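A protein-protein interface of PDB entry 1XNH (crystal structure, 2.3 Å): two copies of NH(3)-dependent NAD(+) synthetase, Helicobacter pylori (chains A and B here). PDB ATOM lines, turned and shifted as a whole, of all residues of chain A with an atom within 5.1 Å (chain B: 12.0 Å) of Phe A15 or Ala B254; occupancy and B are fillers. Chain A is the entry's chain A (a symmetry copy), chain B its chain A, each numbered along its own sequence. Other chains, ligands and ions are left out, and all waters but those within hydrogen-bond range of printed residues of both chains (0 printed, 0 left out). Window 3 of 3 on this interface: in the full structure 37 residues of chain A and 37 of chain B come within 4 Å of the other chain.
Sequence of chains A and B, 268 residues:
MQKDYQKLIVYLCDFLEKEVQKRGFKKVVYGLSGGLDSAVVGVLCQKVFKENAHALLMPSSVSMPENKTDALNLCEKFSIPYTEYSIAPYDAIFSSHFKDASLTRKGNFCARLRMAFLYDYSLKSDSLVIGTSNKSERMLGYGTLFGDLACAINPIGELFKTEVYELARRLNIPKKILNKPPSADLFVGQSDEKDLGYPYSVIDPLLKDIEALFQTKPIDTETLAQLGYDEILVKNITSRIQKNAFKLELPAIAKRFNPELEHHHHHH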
ATOM      1  N   TYR A  11     -24.654 -24.191 -17.722  1.00  0.00           N
ATOM      2  CA  TYR A  11     -24.604 -23.264 -16.601  1.00  0.00           C
ATOM      3  C   TYR A  11     -23.268 -23.325 -15.863  1.00  0.00           C
ATOM      4  O   TYR A  11     -22.604 -22.311 -15.655  1.00  0.00           O
ATOM      5  CB  TYR A  11     -25.742 -23.566 -15.624  1.00  0.00           C
ATOM      6  CG  TYR A  11     -25.685 -22.752 -14.346  1.00  0.00           C
ATOM      7  CD1 TYR A  11     -25.929 -21.381 -14.355  1.00  0.00           C
ATOM      8  CD2 TYR A  11     -25.372 -23.353 -13.134  1.00  0.00           C
ATOM      9  CE1 TYR A  11     -25.863 -20.621 -13.181  1.00  0.00           C
ATOM     10  CE2 TYR A  11     -25.297 -22.611 -11.951  1.00  0.00           C
ATOM     11  CZ  TYR A  11     -25.548 -21.249 -11.981  1.00  0.00           C
ATOM     12  OH  TYR A  11     -25.506 -20.517 -10.809  1.00  0.00           O
ATOM     13  N   LEU A  12     -22.894 -24.535 -15.476  1.00  0.00           N
ATOM     14  CA  LEU A  12     -21.675 -24.782 -14.748  1.00  0.00           C
ATOM     15  C   LEU A  12     -20.426 -24.312 -15.492  1.00  0.00           C
ATOM     16  O   LEU A  12     -19.464 -23.812 -14.900  1.00  0.00           O
ATOM     17  CB  LEU A  12     -21.592 -26.274 -14.419  1.00  0.00           C
ATOM     18  CG  LEU A  12     -22.756 -26.820 -13.595  1.00  0.00           C
ATOM     19  CD1 LEU A  12     -22.301 -28.052 -12.876  1.00  0.00           C
ATOM     20  CD2 LEU A  12     -23.245 -25.796 -12.571  1.00  0.00           C
ATOM     21  N   CYS A  13     -20.447 -24.468 -16.803  1.00  0.00           N
ATOM     22  CA  CYS A  13     -19.327 -24.042 -17.605  1.00  0.00           C
ATOM     23  C   CYS A  13     -19.172 -22.566 -17.515  1.00  0.00           C
ATOM     24  O   CYS A  13     -18.105 -22.049 -17.201  1.00  0.00           O
ATOM     25  CB  CYS A  13     -19.532 -24.438 -19.047  1.00  0.00           C
ATOM     26  SG  CYS A  13     -18.967 -26.112 -19.276  1.00  0.00           S
ATOM     27  N   ASP A  14     -20.255 -21.874 -17.790  1.00  0.00           N
ATOM     28  CA  ASP A  14     -20.201 -20.436 -17.747  1.00  0.00           C
ATOM     29  C   ASP A  14     -19.765 -19.966 -16.355  1.00  0.00           C
ATOM     30  O   ASP A  14     -18.992 -19.015 -16.235  1.00  0.00           O
ATOM     31  CB  ASP A  14     -21.563 -19.891 -18.156  1.00  0.00           C
ATOM     32  CG  ASP A  14     -21.451 -18.725 -19.101  1.00  0.00           C
ATOM     33  OD1 ASP A  14     -21.312 -17.587 -18.602  1.00  0.00           O
ATOM     34  OD2 ASP A  14     -21.489 -18.939 -20.333  1.00  0.00           O
ATOM     35  N   PHE A  15     -20.236 -20.658 -15.315  1.00  0.00           N
ATOM     36  CA  PHE A  15     -19.899 -20.307 -13.929  1.00  0.00           C
ATOM     37  C   PHE A  15     -18.402 -20.442 -13.793  1.00  0.00           C
ATOM     38  O   PHE A  15     -17.738 -19.621 -13.167  1.00  0.00           O
ATOM     39  CB  PHE A  15     -20.624 -21.228 -12.943  1.00  0.00           C
ATOM     40  CG  PHE A  15     -20.179 -21.057 -11.519  1.00  0.00           C
ATOM     41  CD1 PHE A  15     -20.523 -19.925 -10.796  1.00  0.00           C
ATOM     42  CD2 PHE A  15     -19.362 -22.015 -10.920  1.00  0.00           C
ATOM     43  CE1 PHE A  15     -20.056 -19.739  -9.503  1.00  0.00           C
ATOM     44  CE2 PHE A  15     -18.887 -21.842  -9.628  1.00  0.00           C
ATOM     45  CZ  PHE A  15     -19.232 -20.702  -8.915  1.00  0.00           C
ATOM     46  N   LEU A  16     -17.868 -21.496 -14.389  1.00  0.00           N
ATOM     47  CA  LEU A  16     -16.431 -21.694 -14.400  1.00  0.00           C
ATOM     48  C   LEU A  16     -15.680 -20.598 -15.170  1.00  0.00           C
ATOM     49  O   LEU A  16     -14.745 -19.999 -14.648  1.00  0.00           O
ATOM     50  CB  LEU A  16     -16.124 -23.050 -15.015  1.00  0.00           C
ATOM     51  CG  LEU A  16     -16.282 -24.286 -14.103  1.00  0.00           C
ATOM     52  CD1 LEU A  16     -15.975 -25.542 -14.858  1.00  0.00           C
ATOM     53  CD2 LEU A  16     -15.299 -24.127 -13.014  1.00  0.00           C
ATOM     54  N   GLU A  17     -16.055 -20.310 -16.409  1.00  0.00           N
ATOM     55  CA  GLU A  17     -15.305 -19.283 -17.156  1.00  0.00           C
ATOM     56  C   GLU A  17     -15.338 -17.934 -16.458  1.00  0.00           C
ATOM     57  O   GLU A  17     -14.342 -17.192 -16.436  1.00  0.00           O
ATOM     58  CB  GLU A  17     -15.851 -19.152 -18.588  1.00  0.00           C
ATOM     59  CG  GLU A  17     -14.838 -18.591 -19.579  1.00  0.00           C
ATOM     60  CD  GLU A  17     -15.487 -17.918 -20.785  1.00  0.00           C
ATOM     61  OE1 GLU A  17     -16.623 -17.422 -20.650  1.00  0.00           O
ATOM     62  OE2 GLU A  17     -14.850 -17.873 -21.851  1.00  0.00           O
ATOM     63  N   LYS A  18     -16.464 -17.618 -15.837  1.00  0.00           N
ATOM     64  CA  LYS A  18     -16.561 -16.329 -15.161  1.00  0.00           C
ATOM     65  C   LYS A  18     -15.804 -16.206 -13.861  1.00  0.00           C
ATOM     66  O   LYS A  18     -15.238 -15.166 -13.591  1.00  0.00           O
ATOM     67  CB  LYS A  18     -18.018 -15.980 -14.902  1.00  0.00           C
ATOM     68  CG  LYS A  18     -18.738 -15.318 -16.051  1.00  0.00           C
ATOM     69  CD  LYS A  18     -20.092 -14.819 -15.565  1.00  0.00           C
ATOM     70  CE  LYS A  18     -21.271 -15.363 -16.385  1.00  0.00           C
ATOM     71  NZ  LYS A  18     -21.315 -14.834 -17.783  1.00  0.00           N
ATOM     72  N   GLU A  19     -15.814 -17.253 -13.047  1.00  0.00           N
ATOM     73  CA  GLU A  19     -15.143 -17.198 -11.757  1.00  0.00           C
ATOM     74  C   GLU A  19     -13.634 -17.174 -11.842  1.00  0.00           C
ATOM     75  O   GLU A  19     -12.971 -16.353 -11.212  1.00  0.00           O
ATOM     76  CB  GLU A  19     -15.570 -18.382 -10.894  1.00  0.00           C
ATOM     77  CG  GLU A  19     -17.016 -18.372 -10.514  1.00  0.00           C
ATOM     78  CD  GLU A  19     -17.421 -17.094  -9.830  1.00  0.00           C
ATOM     79  OE1 GLU A  19     -16.800 -16.734  -8.813  1.00  0.00           O
ATOM     80  OE2 GLU A  19     -18.347 -16.441 -10.343  1.00  0.00           O
ATOM     81  N   VAL A  20     -13.073 -18.086 -12.612  1.00  0.00           N
ATOM     82  CA  VAL A  20     -11.624 -18.122 -12.717  1.00  0.00           C
ATOM     83  C   VAL A  20     -11.117 -16.811 -13.308  1.00  0.00           C
ATOM     84  O   VAL A  20     -10.096 -16.267 -12.893  1.00  0.00           O
ATOM     85  CB  VAL A  20     -11.179 -19.291 -13.610  1.00  0.00           C
ATOM     86  CG1 VAL A  20      -9.700 -19.200 -13.865  1.00  0.00           C
ATOM     87  CG2 VAL A  20     -11.536 -20.606 -12.934  1.00  0.00           C
ATOM     88  N   ILE A 153     -13.048 -22.239  -5.974  1.00  0.00           N
ATOM     89  CA  ILE A 153     -14.319 -22.350  -6.659  1.00  0.00           C
ATOM     90  C   ILE A 153     -14.753 -23.810  -6.733  1.00  0.00           C
ATOM     91  O   ILE A 153     -13.910 -24.709  -6.867  1.00  0.00           O
ATOM     92  CB  ILE A 153     -14.191 -21.794  -8.083  1.00  0.00           C
ATOM     93  CG1 ILE A 153     -13.809 -20.323  -7.990  1.00  0.00           C
ATOM     94  CG2 ILE A 153     -15.480 -22.028  -8.857  1.00  0.00           C
ATOM     95  CD1 ILE A 153     -13.132 -19.787  -9.242  1.00  0.00           C
ATOM     96  N   ASN A 154     -16.066 -24.032  -6.650  1.00  0.00           N
ATOM     97  CA  ASN A 154     -16.641 -25.376  -6.716  1.00  0.00           C
ATOM     98  C   ASN A 154     -17.899 -25.280  -7.594  1.00  0.00           C
ATOM     99  O   ASN A 154     -18.862 -24.582  -7.219  1.00  0.00           O
ATOM    100  CB  ASN A 154     -17.036 -25.847  -5.306  1.00  0.00           C
ATOM    101  CG  ASN A 154     -17.354 -27.343  -5.249  1.00  0.00           C
ATOM    102  OD1 ASN A 154     -17.828 -27.943  -6.225  1.00  0.00           O
ATOM    103  ND2 ASN A 154     -17.085 -27.945  -4.104  1.00  0.00           N
ATOM    104  N   PRO A 155     -17.911 -25.956  -8.763  1.00  0.00           N
ATOM    105  CA  PRO A 155     -19.019 -25.967  -9.716  1.00  0.00           C
ATOM    106  C   PRO A 155     -20.206 -26.860  -9.400  1.00  0.00           C
ATOM    107  O   PRO A 155     -21.282 -26.692  -9.996  1.00  0.00           O
ATOM    108  CB  PRO A 155     -18.351 -26.438 -10.991  1.00  0.00           C
ATOM    109  CG  PRO A 155     -17.463 -27.490 -10.478  1.00  0.00           C
ATOM    110  CD  PRO A 155     -16.782 -26.710  -9.334  1.00  0.00           C
ATOM    111  N   GLU A 158     -23.623 -27.220  -5.186  1.00  0.00           N
ATOM    112  CA  GLU A 158     -25.040 -27.005  -4.930  1.00  0.00           C
ATOM    113  C   GLU A 158     -25.830 -28.051  -5.703  1.00  0.00           C
ATOM    114  O   GLU A 158     -26.967 -27.823  -6.100  1.00  0.00           O
ATOM    115  CB  GLU A 158     -25.475 -25.594  -5.373  1.00  0.00           C
ATOM    116  CG  GLU A 158     -25.165 -24.527  -4.342  1.00  0.00           C
ATOM    117  CD  GLU A 158     -25.846 -24.852  -3.024  1.00  0.00           C
ATOM    118  OE1 GLU A 158     -27.025 -25.261  -3.095  1.00  0.00           O
ATOM    119  OE2 GLU A 158     -25.226 -24.702  -1.960  1.00  0.00           O
ATOM    120  N   LEU B 250     -15.442 -16.836   1.617  1.00  0.00           N
ATOM    121  CA  LEU B 250     -15.766 -18.234   1.404  1.00  0.00           C
ATOM    122  C   LEU B 250     -15.556 -18.555  -0.066  1.00  0.00           C
ATOM    123  O   LEU B 250     -15.610 -17.671  -0.914  1.00  0.00           O
ATOM    124  CB  LEU B 250     -17.223 -18.499   1.776  1.00  0.00           C
ATOM    125  CG  LEU B 250     -17.579 -18.537   3.264  1.00  0.00           C
ATOM    126  CD1 LEU B 250     -19.087 -18.307   3.417  1.00  0.00           C
ATOM    127  CD2 LEU B 250     -17.127 -19.867   3.864  1.00  0.00           C
ATOM    128  N   PRO B 251     -15.326 -19.840  -0.388  1.00  0.00           N
ATOM    129  CA  PRO B 251     -15.115 -20.245  -1.784  1.00  0.00           C
ATOM    130  C   PRO B 251     -16.317 -19.924  -2.653  1.00  0.00           C
ATOM    131  O   PRO B 251     -17.443 -19.867  -2.169  1.00  0.00           O
ATOM    132  CB  PRO B 251     -14.889 -21.749  -1.674  1.00  0.00           C
ATOM    133  CG  PRO B 251     -15.696 -22.123  -0.459  1.00  0.00           C
ATOM    134  CD  PRO B 251     -15.357 -21.020   0.501  1.00  0.00           C
ATOM    135  N   ALA B 252     -16.074 -19.732  -3.942  1.00  0.00           N
ATOM    136  CA  ALA B 252     -17.145 -19.423  -4.888  1.00  0.00           C
ATOM    137  C   ALA B 252     -17.869 -20.707  -5.296  1.00  0.00           C
ATOM    138  O   ALA B 252     -17.257 -21.651  -5.790  1.00  0.00           O
ATOM    139  CB  ALA B 252     -16.561 -18.734  -6.125  1.00  0.00           C
ATOM    140  N   ILE B 253     -19.178 -20.736  -5.086  1.00  0.00           N
ATOM    141  CA  ILE B 253     -19.985 -21.909  -5.405  1.00  0.00           C
ATOM    142  C   ILE B 253     -21.217 -21.491  -6.194  1.00  0.00           C
ATOM    143  O   ILE B 253     -21.968 -20.611  -5.779  1.00  0.00           O
ATOM    144  CB  ILE B 253     -20.408 -22.633  -4.116  1.00  0.00           C
ATOM    145  CG1 ILE B 253     -19.172 -23.006  -3.310  1.00  0.00           C
ATOM    146  CG2 ILE B 253     -21.176 -23.878  -4.456  1.00  0.00           C
ATOM    147  CD1 ILE B 253     -19.422 -23.152  -1.818  1.00  0.00           C
ATOM    148  N   ALA B 254     -21.409 -22.124  -7.339  1.00  0.00           N
ATOM    149  CA  ALA B 254     -22.537 -21.789  -8.172  1.00  0.00           C
ATOM    150  C   ALA B 254     -23.828 -22.138  -7.415  1.00  0.00           C
ATOM    151  O   ALA B 254     -23.984 -23.252  -6.939  1.00  0.00           O
ATOM    152  CB  ALA B 254     -22.453 -22.554  -9.479  1.00  0.00           C
ATOM    153  N   LYS B 255     -24.724 -21.163  -7.285  1.00  0.00           N
ATOM    154  CA  LYS B 255     -25.988 -21.355  -6.595  1.00  0.00           C
ATOM    155  C   LYS B 255     -26.774 -22.503  -7.222  1.00  0.00           C
ATOM    156  O   LYS B 255     -26.353 -22.973  -8.296  1.00  0.00           O
ATOM    157  CB  LYS B 255     -26.815 -20.080  -6.642  1.00  0.00           C
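The backbone carbonyl oxygen of Ala B252 is in hydrogen-bond range of the backbone NH of Asn A154, at 2.8 Å.
Of the 6 printed residues of chain B, 4 touch a printed residue of chain A. Of the 14 printed residues of chain A, 6 touch a printed residue of chain B. Among the printed residues, 12 pairs touch across the chains. Among the printed residues, no Asp or Glu carboxylate lies within 4 Å of a Lys or Arg side-chain nitrogen of the other chain.
Phe A15 touches just these residues of chain B: Ala B252, Ile B253 and Ala B254. No residue of chain B comes within 4 Å of Cys A13. Lys A18 touches none of the printed residues of chain B. Of chain B, only Ala B252 (3.4 Å) comes within 4 Å of Glu A19. Of chain B, only Ala B252 (3.1 Å) comes within 4 Å of Ile A153. Of chain B, only Ala B252, Ile B253 and Ala B254 come within 4 Å of Asn A154. Of the printed residues of chain A, Ala B252 touches Phe A15 (3.8 Å), Glu A19 (3.4 Å), Ile A153 (3.1 Å) and Asn A154 (2.8 Å). Of the printed residues of chain A, Ile B253 touches Phe A15 (3.5 Å) and Asn A154 (3.4 Å). Printed residues of chain A within 4 Å of Lys B255: Tyr A11 and Glu A158. Pro B251 touches none of the printed residues of chain A. The nearest residue of chain A that does not touch Ala B254 is Pro A155 (4.3 Å). The nearest printed residue of chain A that does not touch Lys B255 is Phe A15 (5.4 Å).
No position is printed for both chains. Of the 12 pairs that touch across the chains among the printed residues, none has its exchanged pair printed and touching as well.
Tyr A11 touches Lys B255. Ala B252 touches Phe A15 (O to CZ, 3.8 Å). Phe A15 touches Ile B253. N of Ala B254 touches CZ of Phe A15, 3.0 Å away. Glu A19 touches Ala B252. Ala B252 touches Ile A153 (O to CA, 3.1 Å). CA of Ile B253 touches O of Asn A154, 3.4 Å away. Ala B254 touches Asn A154. Ala B254 touches Glu A158. Glu A158 touches Lys B255 (CB to C, 3.8 Å).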
